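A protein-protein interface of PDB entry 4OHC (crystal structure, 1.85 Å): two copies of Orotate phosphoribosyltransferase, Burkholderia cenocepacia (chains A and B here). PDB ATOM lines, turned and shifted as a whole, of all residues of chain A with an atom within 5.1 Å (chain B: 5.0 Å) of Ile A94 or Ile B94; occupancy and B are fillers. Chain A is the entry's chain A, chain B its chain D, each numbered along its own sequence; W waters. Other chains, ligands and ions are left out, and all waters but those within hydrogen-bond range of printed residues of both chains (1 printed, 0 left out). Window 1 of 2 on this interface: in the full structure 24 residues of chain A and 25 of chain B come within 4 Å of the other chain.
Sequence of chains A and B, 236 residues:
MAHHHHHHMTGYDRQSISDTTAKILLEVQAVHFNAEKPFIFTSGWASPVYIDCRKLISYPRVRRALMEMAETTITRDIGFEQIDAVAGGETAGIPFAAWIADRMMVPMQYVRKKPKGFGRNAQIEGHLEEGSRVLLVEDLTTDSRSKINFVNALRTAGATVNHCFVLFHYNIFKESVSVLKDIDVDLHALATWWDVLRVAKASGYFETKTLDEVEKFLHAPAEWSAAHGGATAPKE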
ATOM      1  N   GLY A  88     -15.066 -25.043  14.214  1.00  0.00           N
ATOM      2  CA  GLY A  88     -15.874 -23.838  13.939  1.00  0.00           C
ATOM      3  C   GLY A  88     -15.251 -22.882  12.942  1.00  0.00           C
ATOM      4  O   GLY A  88     -14.028 -22.572  13.016  1.00  0.00           O
ATOM      5  N   GLY A  89     -16.037 -22.421  11.978  1.00  0.00           N
ATOM      6  CA  GLY A  89     -15.633 -21.300  11.158  1.00  0.00           C
ATOM      7  C   GLY A  89     -15.596 -19.954  11.891  1.00  0.00           C
ATOM      8  O   GLY A  89     -16.575 -19.539  12.556  1.00  0.00           O
ATOM      9  N   GLU A  90     -14.469 -19.242  11.799  1.00  0.00           N
ATOM     10  CA  GLU A  90     -14.376 -17.899  12.390  1.00  0.00           C
ATOM     11  C   GLU A  90     -15.361 -16.946  11.686  1.00  0.00           C
ATOM     12  O   GLU A  90     -15.437 -16.985  10.444  1.00  0.00           O
ATOM     13  CB  GLU A  90     -12.964 -17.360  12.164  1.00  0.00           C
ATOM     14  CG  GLU A  90     -12.676 -16.067  12.912  1.00  0.00           C
ATOM     15  CD  GLU A  90     -11.366 -15.450  12.509  1.00  0.00           C
ATOM     16  OE1 GLU A  90     -10.936 -15.534  11.310  1.00  0.00           O
ATOM     17  OE2 GLU A  90     -10.760 -14.841  13.432  1.00  0.00           O
ATOM     18  N   THR A  91     -16.119 -16.099  12.404  1.00  0.00           N
ATOM     19  CA  THR A  91     -16.221 -16.050  13.870  1.00  0.00           C
ATOM     20  C   THR A  91     -17.452 -16.725  14.413  1.00  0.00           C
ATOM     21  O   THR A  91     -17.415 -17.386  15.457  1.00  0.00           O
ATOM     22  CB  THR A  91     -16.285 -14.572  14.297  1.00  0.00           C
ATOM     23  OG1 THR A  91     -15.165 -13.904  13.711  1.00  0.00           O
ATOM     24  CG2 THR A  91     -16.120 -14.414  15.727  1.00  0.00           C
ATOM     25  N   ALA A  92     -18.555 -16.550  13.704  1.00  0.00           N
ATOM     26  CA  ALA A  92     -19.883 -16.907  14.235  1.00  0.00           C
ATOM     27  C   ALA A  92     -20.094 -18.387  14.390  1.00  0.00           C
ATOM     28  O   ALA A  92     -20.938 -18.795  15.177  1.00  0.00           O
ATOM     29  CB  ALA A  92     -20.951 -16.309  13.330  1.00  0.00           C
ATOM     30  N   GLY A  93     -19.285 -19.227  13.767  1.00  0.00           N
ATOM     31  CA  GLY A  93     -19.396 -20.643  14.040  1.00  0.00           C
ATOM     32  C   GLY A  93     -18.753 -21.127  15.342  1.00  0.00           C
ATOM     33  O   GLY A  93     -19.068 -22.223  15.830  1.00  0.00           O
ATOM     34  N   ILE A  94     -17.892 -20.295  15.928  1.00  0.00           N
ATOM     35  CA  ILE A  94     -17.076 -20.709  17.079  1.00  0.00           C
ATOM     36  C   ILE A  94     -17.893 -21.056  18.323  1.00  0.00           C
ATOM     37  O   ILE A  94     -17.677 -22.118  18.900  1.00  0.00           O
ATOM     38  CB  ILE A  94     -15.928 -19.727  17.318  1.00  0.00           C
ATOM     39  CG1 ILE A  94     -14.993 -19.716  16.106  1.00  0.00           C
ATOM     40  CG2 ILE A  94     -15.133 -20.097  18.586  1.00  0.00           C
ATOM     41  CD1 ILE A  94     -13.919 -18.670  16.148  1.00  0.00           C
ATOM     42  N   PRO A  95     -18.799 -20.156  18.791  1.00  0.00           N
ATOM     43  CA  PRO A  95     -19.550 -20.580  19.987  1.00  0.00           C
ATOM     44  C   PRO A  95     -20.317 -21.898  19.817  1.00  0.00           C
ATOM     45  O   PRO A  95     -20.337 -22.765  20.720  1.00  0.00           O
ATOM     46  CB  PRO A  95     -20.511 -19.429  20.247  1.00  0.00           C
ATOM     47  CG  PRO A  95     -19.979 -18.225  19.444  1.00  0.00           C
ATOM     48  CD  PRO A  95     -19.209 -18.837  18.295  1.00  0.00           C
ATOM     49  N   PHE A  96     -20.958 -22.053  18.668  1.00  0.00           N
ATOM     50  CA  PHE A  96     -21.727 -23.267  18.383  1.00  0.00           C
ATOM     51  C   PHE A  96     -20.848 -24.478  18.262  1.00  0.00           C
ATOM     52  O   PHE A  96     -21.196 -25.550  18.795  1.00  0.00           O
ATOM     53  CB  PHE A  96     -22.569 -23.082  17.114  1.00  0.00           C
ATOM     54  CG  PHE A  96     -23.472 -21.865  17.202  1.00  0.00           C
ATOM     55  CD1 PHE A  96     -24.508 -21.825  18.150  1.00  0.00           C
ATOM     56  CD2 PHE A  96     -23.256 -20.741  16.409  1.00  0.00           C
ATOM     57  CE1 PHE A  96     -25.297 -20.676  18.266  1.00  0.00           C
ATOM     58  CE2 PHE A  96     -24.083 -19.617  16.504  1.00  0.00           C
ATOM     59  CZ  PHE A  96     -25.089 -19.594  17.450  1.00  0.00           C
ATOM     60  N   ALA A  97     -19.692 -24.311  17.632  1.00  0.00           N
ATOM     61  CA  ALA A  97     -18.713 -25.423  17.592  1.00  0.00           C
ATOM     62  C   ALA A  97     -18.262 -25.805  18.989  1.00  0.00           C
ATOM     63  O   ALA A  97     -18.065 -27.017  19.321  1.00  0.00           O
ATOM     64  CB  ALA A  97     -17.485 -25.025  16.691  1.00  0.00           C
ATOM     65  N   ALA A  98     -18.056 -24.803  19.843  1.00  0.00           N
ATOM     66  CA  ALA A  98     -17.613 -25.081  21.237  1.00  0.00           C
ATOM     67  C   ALA A  98     -18.647 -25.948  22.029  1.00  0.00           C
ATOM     68  O   ALA A  98     -18.266 -26.910  22.704  1.00  0.00           O
ATOM     69  CB  ALA A  98     -17.328 -23.777  22.010  1.00  0.00           C
ATOM     70  N   MET A 108     -12.180 -29.819  19.863  1.00  0.00           N
ATOM     71  CA  MET A 108     -12.553 -28.688  19.039  1.00  0.00           C
ATOM     72  C   MET A 108     -11.319 -28.098  18.333  1.00  0.00           C
ATOM     73  O   MET A 108     -10.220 -28.089  18.860  1.00  0.00           O
ATOM     74  CB  MET A 108     -13.135 -27.614  19.936  1.00  0.00           C
ATOM     75  CG  MET A 108     -13.712 -26.452  19.222  1.00  0.00           C
ATOM     76  SD  MET A 108     -14.156 -25.128  20.329  1.00  0.00           S
ATOM     77  CE  MET A 108     -14.499 -23.902  19.107  1.00  0.00           C
ATOM     78  N   TYR A 110     -10.808 -24.342  15.592  1.00  0.00           N
ATOM     79  CA  TYR A 110     -11.473 -23.371  14.764  1.00  0.00           C
ATOM     80  C   TYR A 110     -10.598 -22.966  13.573  1.00  0.00           C
ATOM     81  O   TYR A 110      -9.401 -23.192  13.581  1.00  0.00           O
ATOM     82  CB  TYR A 110     -12.010 -22.177  15.560  1.00  0.00           C
ATOM     83  CG  TYR A 110     -11.061 -21.248  16.202  1.00  0.00           C
ATOM     84  CD1 TYR A 110     -10.495 -20.151  15.487  1.00  0.00           C
ATOM     85  CD2 TYR A 110     -10.750 -21.365  17.548  1.00  0.00           C
ATOM     86  CE1 TYR A 110      -9.652 -19.254  16.116  1.00  0.00           C
ATOM     87  CE2 TYR A 110      -9.882 -20.477  18.174  1.00  0.00           C
ATOM     88  CZ  TYR A 110      -9.330 -19.428  17.456  1.00  0.00           C
ATOM     89  OH  TYR A 110      -8.542 -18.541  18.088  1.00  0.00           O
ATOM     90  N   GLY B  88     -16.818 -12.722  25.382  1.00  0.00           N
ATOM     91  CA  GLY B  88     -15.494 -13.101  24.972  1.00  0.00           C
ATOM     92  C   GLY B  88     -14.895 -12.117  23.980  1.00  0.00           C
ATOM     93  O   GLY B  88     -15.574 -11.684  23.040  1.00  0.00           O
ATOM     94  N   GLY B  89     -13.604 -11.835  24.137  1.00  0.00           N
ATOM     95  CA  GLY B  89     -12.843 -11.052  23.151  1.00  0.00           C
ATOM     96  C   GLY B  89     -12.541 -11.870  21.900  1.00  0.00           C
ATOM     97  O   GLY B  89     -11.986 -13.007  21.944  1.00  0.00           O
ATOM     98  N   GLU B  90     -12.912 -11.350  20.761  1.00  0.00           N
ATOM     99  CA  GLU B  90     -12.636 -12.048  19.514  1.00  0.00           C
ATOM    100  C   GLU B  90     -11.089 -12.222  19.348  1.00  0.00           C
ATOM    101  O   GLU B  90     -10.366 -11.266  19.709  1.00  0.00           O
ATOM    102  CB  GLU B  90     -13.262 -11.225  18.396  1.00  0.00           C
ATOM    103  CG  GLU B  90     -12.749 -11.458  17.023  1.00  0.00           C
ATOM    104  CD  GLU B  90     -13.406 -10.529  16.005  1.00  0.00           C
ATOM    105  OE1 GLU B  90     -13.095  -9.306  15.996  1.00  0.00           O
ATOM    106  OE2 GLU B  90     -14.190 -11.072  15.168  1.00  0.00           O
ATOM    107  N   THR B  91     -10.554 -13.367  18.880  1.00  0.00           N
ATOM    108  CA  THR B  91     -11.266 -14.634  18.635  1.00  0.00           C
ATOM    109  C   THR B  91     -11.049 -15.695  19.694  1.00  0.00           C
ATOM    110  O   THR B  91     -11.956 -16.464  20.019  1.00  0.00           O
ATOM    111  CB  THR B  91     -10.782 -15.200  17.302  1.00  0.00           C
ATOM    112  OG1 THR B  91     -11.007 -14.188  16.327  1.00  0.00           O
ATOM    113  CG2 THR B  91     -11.552 -16.402  16.873  1.00  0.00           C
ATOM    114  N   ALA B  92      -9.836 -15.726  20.234  1.00  0.00           N
ATOM    115  CA  ALA B  92      -9.414 -16.783  21.133  1.00  0.00           C
ATOM    116  C   ALA B  92     -10.143 -16.795  22.454  1.00  0.00           C
ATOM    117  O   ALA B  92     -10.201 -17.872  23.096  1.00  0.00           O
ATOM    118  CB  ALA B  92      -7.887 -16.687  21.341  1.00  0.00           C
ATOM    119  N   GLY B  93     -10.762 -15.674  22.847  1.00  0.00           N
ATOM    120  CA  GLY B  93     -11.622 -15.635  24.008  1.00  0.00           C
ATOM    121  C   GLY B  93     -12.965 -16.363  23.860  1.00  0.00           C
ATOM    122  O   GLY B  93     -13.606 -16.711  24.826  1.00  0.00           O
ATOM    123  N   ILE B  94     -13.406 -16.568  22.631  1.00  0.00           N
ATOM    124  CA  ILE B  94     -14.762 -16.970  22.361  1.00  0.00           C
ATOM    125  C   ILE B  94     -15.118 -18.386  22.861  1.00  0.00           C
ATOM    126  O   ILE B  94     -16.183 -18.599  23.417  1.00  0.00           O
ATOM    127  CB  ILE B  94     -15.090 -16.717  20.874  1.00  0.00           C
ATOM    128  CG1 ILE B  94     -15.103 -15.194  20.622  1.00  0.00           C
ATOM    129  CG2 ILE B  94     -16.462 -17.271  20.490  1.00  0.00           C
ATOM    130  CD1 ILE B  94     -15.359 -14.821  19.151  1.00  0.00           C
ATOM    131  N   PRO B  95     -14.276 -19.365  22.603  1.00  0.00           N
ATOM    132  CA  PRO B  95     -14.669 -20.696  23.080  1.00  0.00           C
ATOM    133  C   PRO B  95     -14.792 -20.726  24.596  1.00  0.00           C
ATOM    134  O   PRO B  95     -15.738 -21.346  25.114  1.00  0.00           O
ATOM    135  CB  PRO B  95     -13.511 -21.607  22.618  1.00  0.00           C
ATOM    136  CG  PRO B  95     -12.864 -20.842  21.507  1.00  0.00           C
ATOM    137  CD  PRO B  95     -13.035 -19.385  21.833  1.00  0.00           C
ATOM    138  N   PHE B  96     -13.825 -20.122  25.284  1.00  0.00           N
ATOM    139  CA  PHE B  96     -13.780 -20.123  26.754  1.00  0.00           C
ATOM    140  C   PHE B  96     -14.990 -19.328  27.245  1.00  0.00           C
ATOM    141  O   PHE B  96     -15.631 -19.719  28.187  1.00  0.00           O
ATOM    142  CB  PHE B  96     -12.469 -19.543  27.242  1.00  0.00           C
ATOM    143  CG  PHE B  96     -11.280 -20.299  26.680  1.00  0.00           C
ATOM    144  CD1 PHE B  96     -11.128 -21.663  26.965  1.00  0.00           C
ATOM    145  CD2 PHE B  96     -10.386 -19.696  25.812  1.00  0.00           C
ATOM    146  CE1 PHE B  96     -10.087 -22.399  26.399  1.00  0.00           C
ATOM    147  CE2 PHE B  96      -9.351 -20.439  25.267  1.00  0.00           C
ATOM    148  CZ  PHE B  96      -9.192 -21.774  25.592  1.00  0.00           C
ATOM    149  N   ALA B  97     -15.326 -18.235  26.600  1.00  0.00           N
ATOM    150  CA  ALA B  97     -16.534 -17.492  27.022  1.00  0.00           C
ATOM    151  C   ALA B  97     -17.836 -18.311  26.836  1.00  0.00           C
ATOM    152  O   ALA B  97     -18.736 -18.265  27.658  1.00  0.00           O
ATOM    153  CB  ALA B  97     -16.619 -16.175  26.270  1.00  0.00           C
ATOM    154  N   ALA B  98     -17.914 -19.065  25.736  1.00  0.00           N
ATOM    155  CA  ALA B  98     -19.048 -19.944  25.481  1.00  0.00           C
ATOM    156  C   ALA B  98     -19.218 -20.965  26.632  1.00  0.00           C
ATOM    157  O   ALA B  98     -20.333 -21.179  27.134  1.00  0.00           O
ATOM    158  CB  ALA B  98     -18.918 -20.661  24.137  1.00  0.00           C
ATOM    159  N   MET B 108     -24.368 -14.974  26.714  1.00  0.00           N
ATOM    160  CA  MET B 108     -23.054 -14.732  26.177  1.00  0.00           C
ATOM    161  C   MET B 108     -23.155 -13.608  25.095  1.00  0.00           C
ATOM    162  O   MET B 108     -24.153 -13.494  24.441  1.00  0.00           O
ATOM    163  CB  MET B 108     -22.603 -15.997  25.459  1.00  0.00           C
ATOM    164  CG  MET B 108     -21.293 -15.890  24.724  1.00  0.00           C
ATOM    165  SD  MET B 108     -20.852 -17.360  23.820  1.00  0.00           S
ATOM    166  CE  MET B 108     -19.248 -16.718  23.152  1.00  0.00           C
ATOM    167  N   TYR B 110     -20.035 -11.657  22.252  1.00  0.00           N
ATOM    168  CA  TYR B 110     -18.616 -11.483  21.991  1.00  0.00           C
ATOM    169  C   TYR B 110     -18.344 -10.088  21.451  1.00  0.00           C
ATOM    170  O   TYR B 110     -19.241  -9.383  21.000  1.00  0.00           O
ATOM    171  CB  TYR B 110     -18.034 -12.590  21.124  1.00  0.00           C
ATOM    172  CG  TYR B 110     -18.507 -12.777  19.691  1.00  0.00           C
ATOM    173  CD1 TYR B 110     -17.947 -12.026  18.621  1.00  0.00           C
ATOM    174  CD2 TYR B 110     -19.430 -13.764  19.370  1.00  0.00           C
ATOM    175  CE1 TYR B 110     -18.334 -12.267  17.297  1.00  0.00           C
ATOM    176  CE2 TYR B 110     -19.835 -13.977  18.053  1.00  0.00           C
ATOM    177  CZ  TYR B 110     -19.289 -13.267  17.027  1.00  0.00           C
ATOM    178  OH  TYR B 110     -19.686 -13.521  15.688  1.00  0.00           O
HETATM  179  O   HOH W   1     -16.850 -11.065  13.987  1.00  0.00           O
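The side-chain carboxylate (OE2) of Glu A90 lies within hydrogen-bond range of the side-chain hydroxyl (OG1) of Thr B91 (3.0 Å).
OE2 of Glu B90 is in hydrogen-bond range of OG1 of Thr A91, 3.3 Å away.
Thr A91 touches Ile B94, and with the chains exchanged Ile A94 touches Thr B91.
Ala A92 touches Tyr B110, and with the chains exchanged Tyr A110 touches Ala B92.
Ile B94 touches its own counterpart, Ile A94.
Ile A94 touches Pro B95, and with the chains exchanged Pro A95 touches Ile B94.
Of the 11 pairs that touch across the chains among the printed residues, 11 have their exchanged pair printed and touching as well.
CG2 of Thr A91 touches CD1 of Ile B94, 3.5 Å away.
Thr A91 touches Tyr B110.
Ala A92 touches Tyr B110.
Thr B91 touches Ile A94 (CG2 to CD1, 3.4 Å).
Ile B94 touches Ile A94 (CG2 to CG2, 3.7 Å).
CG2 of Ile A94 touches CG of Pro B95, 3.8 Å away.
CG2 of Ile B94 touches CG of Pro A95, 3.8 Å away.
Thr B91 touches Tyr A110 (CG2 to CE1, 3.5 Å).
OH of Tyr A110 touches CA of Ala B92, 3.6 Å away.
Water W1 lies within hydrogen-bond range of the side-chain carboxylate (OE2) of Glu B90 (2.9 Å) and the side-chain hydroxyl (OG1) of Thr A91 (3.3 Å).
Printed residues of chain A that touch a printed residue of chain B: Glu A90, Thr A91, Ala A92, Ile A94, Pro A95 and Tyr A110.
Hydrophobic or aromatic side chains of chain A that line the printed part of chain B: Ala A92, Ile A94, Pro A95 and Tyr A110.
Printed residues of chain B that touch a printed residue of chain A: Glu B90, Thr B91, Ala B92, Ile B94, Pro B95 and Tyr B110.
Among the printed residues, no Asp or Glu carboxylate lies within 4 Å of a Lys or Arg side-chain nitrogen of the other chain.
Of the printed residues of chain B, Glu A90 touches Thr B91 (3.0 Å).
Of chain B, only Thr B91 (3.4 Å), Ile B94 (3.7 Å) and Pro B95 (3.8 Å) come within 4 Å of Ile A94.
Printed residues of chain B within 4 Å of Pro A95: Ile B94.
Printed residues of chain B within 4 Å of Tyr A110: Thr B91 and Ala B92.
Of the printed residues of chain A, Thr B91 touches Glu A90, Ile A94 and Tyr A110.
Of chain A, only Thr A91, Ile A94 and Pro A95 come within 4 Å of Ile B94.
Printed residues of chain A within 4 Å of Pro B95: Ile A94.
Phe B96 touches none of the printed residues of chain A.
Ala B98 touches none of the printed residues of chain A.
The nearest printed residue of chain B that does not touch Tyr A110 is Pro B95 (4.5 Å).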
